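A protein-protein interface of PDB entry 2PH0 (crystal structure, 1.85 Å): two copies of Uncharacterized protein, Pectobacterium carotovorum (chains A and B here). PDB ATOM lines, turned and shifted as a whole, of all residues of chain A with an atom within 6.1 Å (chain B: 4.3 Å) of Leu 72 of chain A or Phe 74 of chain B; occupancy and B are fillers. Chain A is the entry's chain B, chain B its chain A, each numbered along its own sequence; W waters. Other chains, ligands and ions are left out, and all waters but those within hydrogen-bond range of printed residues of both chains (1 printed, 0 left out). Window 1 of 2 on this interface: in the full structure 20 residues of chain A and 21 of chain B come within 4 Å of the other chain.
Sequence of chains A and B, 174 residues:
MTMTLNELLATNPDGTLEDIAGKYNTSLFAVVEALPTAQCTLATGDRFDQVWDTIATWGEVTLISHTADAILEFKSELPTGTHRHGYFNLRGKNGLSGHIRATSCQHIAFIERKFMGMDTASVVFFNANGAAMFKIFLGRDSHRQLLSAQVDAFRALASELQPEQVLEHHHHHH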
ATOM      1  N   LEU A  63     -13.572 -18.482   8.796  1.00  0.00           N
ATOM      2  CA  LEU A  63     -13.099 -19.531   7.893  1.00  0.00           C
ATOM      3  C   LEU A  63     -12.941 -18.864   6.537  1.00  0.00           C
ATOM      4  O   LEU A  63     -13.826 -18.139   6.089  1.00  0.00           O
ATOM      5  CB  LEU A  63     -14.098 -20.691   7.810  1.00  0.00           C
ATOM      6  CG  LEU A  63     -13.641 -21.845   6.907  1.00  0.00           C
ATOM      7  CD1 LEU A  63     -14.194 -23.162   7.420  1.00  0.00           C
ATOM      8  CD2 LEU A  63     -14.093 -21.587   5.478  1.00  0.00           C
ATOM      9  N   ILE A  64     -11.811 -19.103   5.887  1.00  0.00           N
ATOM     10  CA  ILE A  64     -11.529 -18.467   4.609  1.00  0.00           C
ATOM     11  C   ILE A  64     -11.084 -19.453   3.547  1.00  0.00           C
ATOM     12  O   ILE A  64     -10.304 -20.367   3.825  1.00  0.00           O
ATOM     13  CB  ILE A  64     -10.391 -17.419   4.759  1.00  0.00           C
ATOM     14  CG1 ILE A  64     -10.824 -16.300   5.704  1.00  0.00           C
ATOM     15  CG2 ILE A  64     -10.003 -16.853   3.391  1.00  0.00           C
ATOM     16  CD1 ILE A  64      -9.731 -15.284   5.982  1.00  0.00           C
ATOM     17  N   SER A  65     -11.610 -19.267   2.340  1.00  0.00           N
ATOM     18  CA  SER A  65     -11.228 -20.071   1.188  1.00  0.00           C
ATOM     19  C   SER A  65     -10.411 -19.063   0.388  1.00  0.00           C
ATOM     20  O   SER A  65     -10.922 -18.006   0.026  1.00  0.00           O
ATOM     21  CB  SER A  65     -12.447 -20.485   0.369  1.00  0.00           C
ATOM     22  OG  SER A  65     -12.021 -21.176  -0.791  1.00  0.00           O
ATOM     23  N   HIS A  66      -9.151 -19.378   0.114  1.00  0.00           N
ATOM     24  CA  HIS A  66      -8.301 -18.436  -0.599  1.00  0.00           C
ATOM     25  C   HIS A  66      -7.677 -19.023  -1.855  1.00  0.00           C
ATOM     26  O   HIS A  66      -6.836 -19.921  -1.782  1.00  0.00           O
ATOM     27  CB  HIS A  66      -7.199 -17.938   0.343  1.00  0.00           C
ATOM     28  CG  HIS A  66      -6.380 -16.816  -0.214  1.00  0.00           C
ATOM     29  ND1 HIS A  66      -5.872 -16.826  -1.494  1.00  0.00           N
ATOM     30  CD2 HIS A  66      -5.963 -15.654   0.346  1.00  0.00           C
ATOM     31  CE1 HIS A  66      -5.181 -15.720  -1.702  1.00  0.00           C
ATOM     32  NE2 HIS A  66      -5.221 -14.991  -0.601  1.00  0.00           N
ATOM     33  N   ALA A  70     -10.769 -16.165  -6.131  1.00  0.00           N
ATOM     34  CA  ALA A  70     -11.704 -15.722  -5.115  1.00  0.00           C
ATOM     35  C   ALA A  70     -11.249 -16.006  -3.703  1.00  0.00           C
ATOM     36  O   ALA A  70     -10.751 -17.087  -3.393  1.00  0.00           O
ATOM     37  CB  ALA A  70     -13.067 -16.360  -5.347  1.00  0.00           C
ATOM     38  N   ILE A  71     -11.426 -15.009  -2.851  1.00  0.00           N
ATOM     39  CA  ILE A  71     -11.110 -15.129  -1.440  1.00  0.00           C
ATOM     40  C   ILE A  71     -12.469 -14.984  -0.759  1.00  0.00           C
ATOM     41  O   ILE A  71     -13.094 -13.927  -0.830  1.00  0.00           O
ATOM     42  CB  ILE A  71     -10.170 -14.004  -0.969  1.00  0.00           C
ATOM     43  CG1 ILE A  71      -8.844 -14.081  -1.735  1.00  0.00           C
ATOM     44  CG2 ILE A  71      -9.935 -14.127   0.526  1.00  0.00           C
ATOM     45  CD1 ILE A  71      -7.876 -12.951  -1.419  1.00  0.00           C
ATOM     46  N   LEU A  72     -12.940 -16.056  -0.132  1.00  0.00           N
ATOM     47  CA  LEU A  72     -14.235 -16.038   0.542  1.00  0.00           C
ATOM     48  C   LEU A  72     -14.029 -16.163   2.048  1.00  0.00           C
ATOM     49  O   LEU A  72     -13.354 -17.076   2.521  1.00  0.00           O
ATOM     50  CB  LEU A  72     -15.094 -17.182   0.017  1.00  0.00           C
ATOM     51  CG  LEU A  72     -15.251 -17.118  -1.505  1.00  0.00           C
ATOM     52  CD1 LEU A  72     -16.012 -18.337  -1.995  1.00  0.00           C
ATOM     53  CD2 LEU A  72     -15.986 -15.823  -1.885  1.00  0.00           C
ATOM     54  N   GLU A  73     -14.606 -15.232   2.800  1.00  0.00           N
ATOM     55  CA  GLU A  73     -14.439 -15.225   4.248  1.00  0.00           C
ATOM     56  C   GLU A  73     -15.773 -15.328   4.967  1.00  0.00           C
ATOM     57  O   GLU A  73     -16.736 -14.680   4.585  1.00  0.00           O
ATOM     58  CB  GLU A  73     -13.745 -13.938   4.673  1.00  0.00           C
ATOM     59  CG  GLU A  73     -12.474 -13.646   3.919  1.00  0.00           C
ATOM     60  CD  GLU A  73     -11.966 -12.249   4.190  1.00  0.00           C
ATOM     61  OE1 GLU A  73     -12.000 -11.824   5.365  1.00  0.00           O
ATOM     62  OE2 GLU A  73     -11.530 -11.581   3.229  1.00  0.00           O
ATOM     63  N   PHE A  74     -15.826 -16.136   6.018  1.00  0.00           N
ATOM     64  CA  PHE A  74     -17.069 -16.285   6.759  1.00  0.00           C
ATOM     65  C   PHE A  74     -16.842 -16.357   8.251  1.00  0.00           C
ATOM     66  O   PHE A  74     -16.145 -17.247   8.736  1.00  0.00           O
ATOM     67  CB  PHE A  74     -17.812 -17.533   6.309  1.00  0.00           C
ATOM     68  CG  PHE A  74     -19.257 -17.538   6.714  1.00  0.00           C
ATOM     69  CD1 PHE A  74     -19.659 -18.118   7.914  1.00  0.00           C
ATOM     70  CD2 PHE A  74     -20.216 -16.922   5.912  1.00  0.00           C
ATOM     71  CE1 PHE A  74     -20.994 -18.083   8.311  1.00  0.00           C
ATOM     72  CE2 PHE A  74     -21.556 -16.880   6.302  1.00  0.00           C
ATOM     73  CZ  PHE A  74     -21.943 -17.463   7.505  1.00  0.00           C
ATOM     74  N   GLY A  95     -25.061 -20.462   9.277  1.00  0.00           N
ATOM     75  CA  GLY A  95     -24.773 -20.029   7.919  1.00  0.00           C
ATOM     76  C   GLY A  95     -23.627 -20.754   7.244  1.00  0.00           C
ATOM     77  O   GLY A  95     -23.458 -20.660   6.032  1.00  0.00           O
ATOM     78  N   LEU A  96     -22.829 -21.474   8.025  1.00  0.00           N
ATOM     79  CA  LEU A  96     -21.698 -22.205   7.468  1.00  0.00           C
ATOM     80  C   LEU A  96     -21.928 -23.708   7.506  1.00  0.00           C
ATOM     81  O   LEU A  96     -22.197 -24.272   8.562  1.00  0.00           O
ATOM     82  CB  LEU A  96     -20.422 -21.873   8.244  1.00  0.00           C
ATOM     83  CG  LEU A  96     -19.156 -22.658   7.891  1.00  0.00           C
ATOM     84  CD1 LEU A  96     -18.769 -22.408   6.443  1.00  0.00           C
ATOM     85  CD2 LEU A  96     -18.023 -22.231   8.820  1.00  0.00           C
ATOM     86  N   SER A  97     -21.836 -24.351   6.348  1.00  0.00           N
ATOM     87  CA  SER A  97     -21.996 -25.795   6.265  1.00  0.00           C
ATOM     88  C   SER A  97     -21.089 -26.297   5.151  1.00  0.00           C
ATOM     89  O   SER A  97     -20.289 -25.533   4.609  1.00  0.00           O
ATOM     90  CB  SER A  97     -23.453 -26.181   5.985  1.00  0.00           C
ATOM     91  OG  SER A  97     -23.910 -25.648   4.753  1.00  0.00           O
ATOM     92  N   VAL B  61     -29.319 -16.655  -0.174  1.00  0.00           N
ATOM     93  CA  VAL B  61     -28.901 -17.675  -1.132  1.00  0.00           C
ATOM     94  C   VAL B  61     -27.687 -18.375  -0.524  1.00  0.00           C
ATOM     95  O   VAL B  61     -27.214 -17.976   0.542  1.00  0.00           O
ATOM     96  CB  VAL B  61     -28.513 -17.063  -2.507  1.00  0.00           C
ATOM     97  CG1 VAL B  61     -29.735 -16.385  -3.146  1.00  0.00           C
ATOM     98  CG2 VAL B  61     -27.377 -16.065  -2.347  1.00  0.00           C
ATOM     99  N   THR B  62     -27.194 -19.429  -1.166  1.00  0.00           N
ATOM    100  CA  THR B  62     -26.019 -20.117  -0.641  1.00  0.00           C
ATOM    101  C   THR B  62     -24.849 -19.978  -1.608  1.00  0.00           C
ATOM    102  O   THR B  62     -24.917 -20.434  -2.745  1.00  0.00           O
ATOM    103  CB  THR B  62     -26.281 -21.613  -0.402  1.00  0.00           C
ATOM    104  OG1 THR B  62     -27.486 -21.767   0.354  1.00  0.00           O
ATOM    105  CG2 THR B  62     -25.133 -22.232   0.397  1.00  0.00           C
ATOM    106  N   LEU B  63     -23.792 -19.315  -1.150  1.00  0.00           N
ATOM    107  CA  LEU B  63     -22.581 -19.127  -1.948  1.00  0.00           C
ATOM    108  C   LEU B  63     -21.708 -20.333  -1.624  1.00  0.00           C
ATOM    109  O   LEU B  63     -21.479 -20.634  -0.454  1.00  0.00           O
ATOM    110  CB  LEU B  63     -21.868 -17.845  -1.528  1.00  0.00           C
ATOM    111  CG  LEU B  63     -20.597 -17.461  -2.281  1.00  0.00           C
ATOM    112  CD1 LEU B  63     -20.970 -16.894  -3.636  1.00  0.00           C
ATOM    113  CD2 LEU B  63     -19.818 -16.431  -1.476  1.00  0.00           C
ATOM    114  N   SER B  65     -18.049 -22.703  -2.413  1.00  0.00           N
ATOM    115  CA  SER B  65     -16.719 -22.895  -2.975  1.00  0.00           C
ATOM    116  C   SER B  65     -16.670 -24.413  -3.083  1.00  0.00           C
ATOM    117  O   SER B  65     -16.819 -25.111  -2.080  1.00  0.00           O
ATOM    118  CB  SER B  65     -15.628 -22.413  -2.017  1.00  0.00           C
ATOM    119  OG  SER B  65     -14.405 -23.037  -2.351  1.00  0.00           O
ATOM    120  N   LEU B  72     -17.538 -25.795   0.626  1.00  0.00           N
ATOM    121  CA  LEU B  72     -17.838 -24.863   1.706  1.00  0.00           C
ATOM    122  C   LEU B  72     -19.057 -24.064   1.294  1.00  0.00           C
ATOM    123  O   LEU B  72     -19.073 -23.459   0.216  1.00  0.00           O
ATOM    124  CB  LEU B  72     -16.636 -23.950   1.939  1.00  0.00           C
ATOM    125  CG  LEU B  72     -15.367 -24.762   2.227  1.00  0.00           C
ATOM    126  CD1 LEU B  72     -14.149 -23.850   2.274  1.00  0.00           C
ATOM    127  CD2 LEU B  72     -15.545 -25.538   3.526  1.00  0.00           C
ATOM    128  N   GLU B  73     -20.079 -24.063   2.150  1.00  0.00           N
ATOM    129  CA  GLU B  73     -21.336 -23.370   1.839  1.00  0.00           C
ATOM    130  C   GLU B  73     -21.614 -22.256   2.834  1.00  0.00           C
ATOM    131  O   GLU B  73     -21.631 -22.486   4.044  1.00  0.00           O
ATOM    132  CB  GLU B  73     -22.481 -24.386   1.841  1.00  0.00           C
ATOM    133  CG  GLU B  73     -22.103 -25.692   1.161  1.00  0.00           C
ATOM    134  CD  GLU B  73     -23.190 -26.744   1.247  1.00  0.00           C
ATOM    135  OE1 GLU B  73     -23.691 -27.008   2.360  1.00  0.00           O
ATOM    136  OE2 GLU B  73     -23.539 -27.310   0.196  1.00  0.00           O
ATOM    137  N   PHE B  74     -21.836 -21.052   2.309  1.00  0.00           N
ATOM    138  CA  PHE B  74     -22.082 -19.869   3.128  1.00  0.00           C
ATOM    139  C   PHE B  74     -23.481 -19.335   2.800  1.00  0.00           C
ATOM    140  O   PHE B  74     -23.705 -18.823   1.711  1.00  0.00           O
ATOM    141  CB  PHE B  74     -21.036 -18.785   2.804  1.00  0.00           C
ATOM    142  CG  PHE B  74     -19.597 -19.278   2.785  1.00  0.00           C
ATOM    143  CD1 PHE B  74     -18.985 -19.755   3.944  1.00  0.00           C
ATOM    144  CD2 PHE B  74     -18.848 -19.228   1.612  1.00  0.00           C
ATOM    145  CE1 PHE B  74     -17.643 -20.171   3.935  1.00  0.00           C
ATOM    146  CE2 PHE B  74     -17.510 -19.639   1.590  1.00  0.00           C
ATOM    147  CZ  PHE B  74     -16.908 -20.113   2.761  1.00  0.00           C
ATOM    148  N   LYS B  75     -24.419 -19.453   3.735  1.00  0.00           N
ATOM    149  CA  LYS B  75     -25.783 -18.994   3.500  1.00  0.00           C
ATOM    150  C   LYS B  75     -25.992 -17.545   3.938  1.00  0.00           C
ATOM    151  O   LYS B  75     -25.763 -17.200   5.100  1.00  0.00           O
ATOM    152  CB  LYS B  75     -26.766 -19.915   4.243  1.00  0.00           C
ATOM    153  CG  LYS B  75     -28.222 -19.739   3.861  1.00  0.00           C
ATOM    154  CD  LYS B  75     -29.136 -20.628   4.697  1.00  0.00           C
ATOM    155  CE  LYS B  75     -28.875 -22.110   4.458  1.00  0.00           C
ATOM    156  NZ  LYS B  75     -29.785 -22.978   5.267  1.00  0.00           N
ATOM    157  N   SER B  76     -26.415 -16.694   3.007  1.00  0.00           N
ATOM    158  CA  SER B  76     -26.678 -15.292   3.325  1.00  0.00           C
ATOM    159  C   SER B  76     -27.141 -14.512   2.107  1.00  0.00           C
ATOM    160  O   SER B  76     -27.184 -15.036   0.996  1.00  0.00           O
ATOM    161  CB  SER B  76     -25.426 -14.614   3.895  1.00  0.00           C
ATOM    162  OG  SER B  76     -24.354 -14.650   2.969  1.00  0.00           O
ATOM    163  N   LEU B  96     -20.496 -12.811   5.753  1.00  0.00           N
ATOM    164  CA  LEU B  96     -19.845 -13.135   4.483  1.00  0.00           C
ATOM    165  C   LEU B  96     -19.149 -11.939   3.848  1.00  0.00           C
ATOM    166  O   LEU B  96     -19.776 -10.914   3.585  1.00  0.00           O
ATOM    167  CB  LEU B  96     -20.868 -13.703   3.492  1.00  0.00           C
ATOM    168  CG  LEU B  96     -20.365 -13.975   2.070  1.00  0.00           C
ATOM    169  CD1 LEU B  96     -19.275 -15.038   2.092  1.00  0.00           C
ATOM    170  CD2 LEU B  96     -21.526 -14.422   1.194  1.00  0.00           C
ATOM    171  N   SER B  97     -17.848 -12.074   3.607  1.00  0.00           N
ATOM    172  CA  SER B  97     -17.065 -11.012   2.983  1.00  0.00           C
ATOM    173  C   SER B  97     -16.022 -11.648   2.070  1.00  0.00           C
ATOM    174  O   SER B  97     -15.972 -12.869   1.928  1.00  0.00           O
ATOM    175  CB  SER B  97     -16.382 -10.155   4.050  1.00  0.00           C
ATOM    176  OG  SER B  97     -15.390 -10.887   4.746  1.00  0.00           O
HETATM  177  O   HOH W   1     -24.786 -23.151   4.801  1.00  0.00           O
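O of Glu 73 of chain B sits close to O of Gly 95 of chain A (3.3 Å). The backbone carbonyl oxygen (O) of Ser 97 of chain B is in hydrogen-bond range of the backbone NH (N) of Glu 73 of chain A, 2.9 Å away. The side-chain hydroxyl (OG) of Ser 65 of chain B is in hydrogen-bond range of the side-chain hydroxyl (OG) of Ser 65 of chain A, at 3.4 Å. The side-chain hydroxyl (OG) of Ser 97 of chain A lies within hydrogen-bond range of the side-chain carboxylate (OE1) of Glu 73 of chain B (2.8 Å). The backbone NH of Lys 75 of chain B is in hydrogen-bond range of the backbone carbonyl oxygen of Gly 95 of chain A (2.8 Å).
O of Leu 72 of chain A lies within hydrogen-bond range of N of Ser 65 of chain A. N of Leu 72 of chain B sits at hydrogen-bond distance from O of Ser 65 of chain B. O of Leu 63 of chain B is in hydrogen-bond range of N of Phe 74 of chain B (2.8 Å). O of Leu 63 of chain A is in hydrogen-bond range of N of Phe 74 of chain A, 2.8 Å away.
CD1 of Leu 72 of chain B touches CD2 of Leu 63 of chain A, 3.9 Å away. Leu 72 of chain A touches Leu 63 of chain B. CE2 of Phe 74 of chain B touches CB of Leu 72 of chain A (3.8 Å). C of Leu 72 of chain A touches O of Ser 97 of chain B (3.8 Å). Leu 96 of chain B touches Glu 73 of chain A (CA to O, 3.5 Å). Phe 74 of chain B touches Phe 74 of chain A (CD1 to CB, 3.5 Å). CA of Phe 74 of chain B touches O of Gly 95 of chain A, 3.3 Å away. Glu 73 of chain B touches Leu 96 of chain A. CD1 of Leu 96 of chain A touches CE1 of Phe 74 of chain B, at 3.5 Å. Ser 97 of chain A touches Leu 72 of chain B (O to C, 3.8 Å).
Leu 72 of chain A touches just these residues of chain B: Leu 63, Phe 74 and Ser 97. Phe 74 of chain B touches just these residues of chain A: Leu 72 (3.8 Å), Phe 74 (3.5 Å), Gly 95 (3.3 Å) and Leu 96 (3.5 Å). Printed residues of chain A within 4 Å of Leu 63 of chain B: Leu 72. Of the printed residues of chain A, Leu 96 of chain B touches Glu 73 (3.5 Å). Of the printed residues of chain A, Ser 97 of chain B touches Leu 72 (3.8 Å) and Glu 73 (2.9 Å). Of the printed residues of chain B, Glu 73 of chain A touches Leu 96 (3.5 Å) and Ser 97 (2.9 Å). Printed residues of chain A within 4 Å of Lys 75 of chain B: Gly 95 (2.8 Å). The nearest residue of chain B that does not touch Leu 72 of chain A is Ser 65 of chain B (4.1 Å). The nearest residue of chain A that does not touch Phe 74 of chain B is Leu 63 of chain A (4.1 Å).
Hydrophobic or aromatic side chains of chain B that line the printed part of chain A: Leu 63, Leu 72, Phe 74 and Leu 96. Of the 12 printed residues of chain A, 8 touch a printed residue of chain B. Among the printed residues, 15 pairs touch across the chains. Among the printed residues, no Asp or Glu carboxylate lies within 4 Å of a Lys or Arg side-chain nitrogen of the other chain.
Leu 63 of chain A touches Leu 72 of chain B, and with the chains exchanged Leu 72 of chain A touches Leu 63 of chain B. Leu 72 of chain A touches Ser 97 of chain B, and with the chains exchanged Ser 97 of chain A touches Leu 72 of chain B. Glu 73 of chain A touches Ser 97 of chain B, and with the chains exchanged Ser 97 of chain A touches Glu 73 of chain B. Leu 96 of chain A touches Phe 74 of chain B, but with the chains exchanged Phe 74 of chain A does not touch Leu 96 of chain B (4.1 Å). Positions printed for both chains: 63, 65, 72, 73, 74, 96 and 97. Of the 15 pairs that touch across the chains among the printed residues, 10 have their exchanged pair printed and touching as well.
Water W1 lies within hydrogen-bond range of OG of Ser 97 of chain A (2.6 Å), O of Gly 95 of chain A (3.1 Å) and O of Glu 73 of chain B (3.3 Å).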
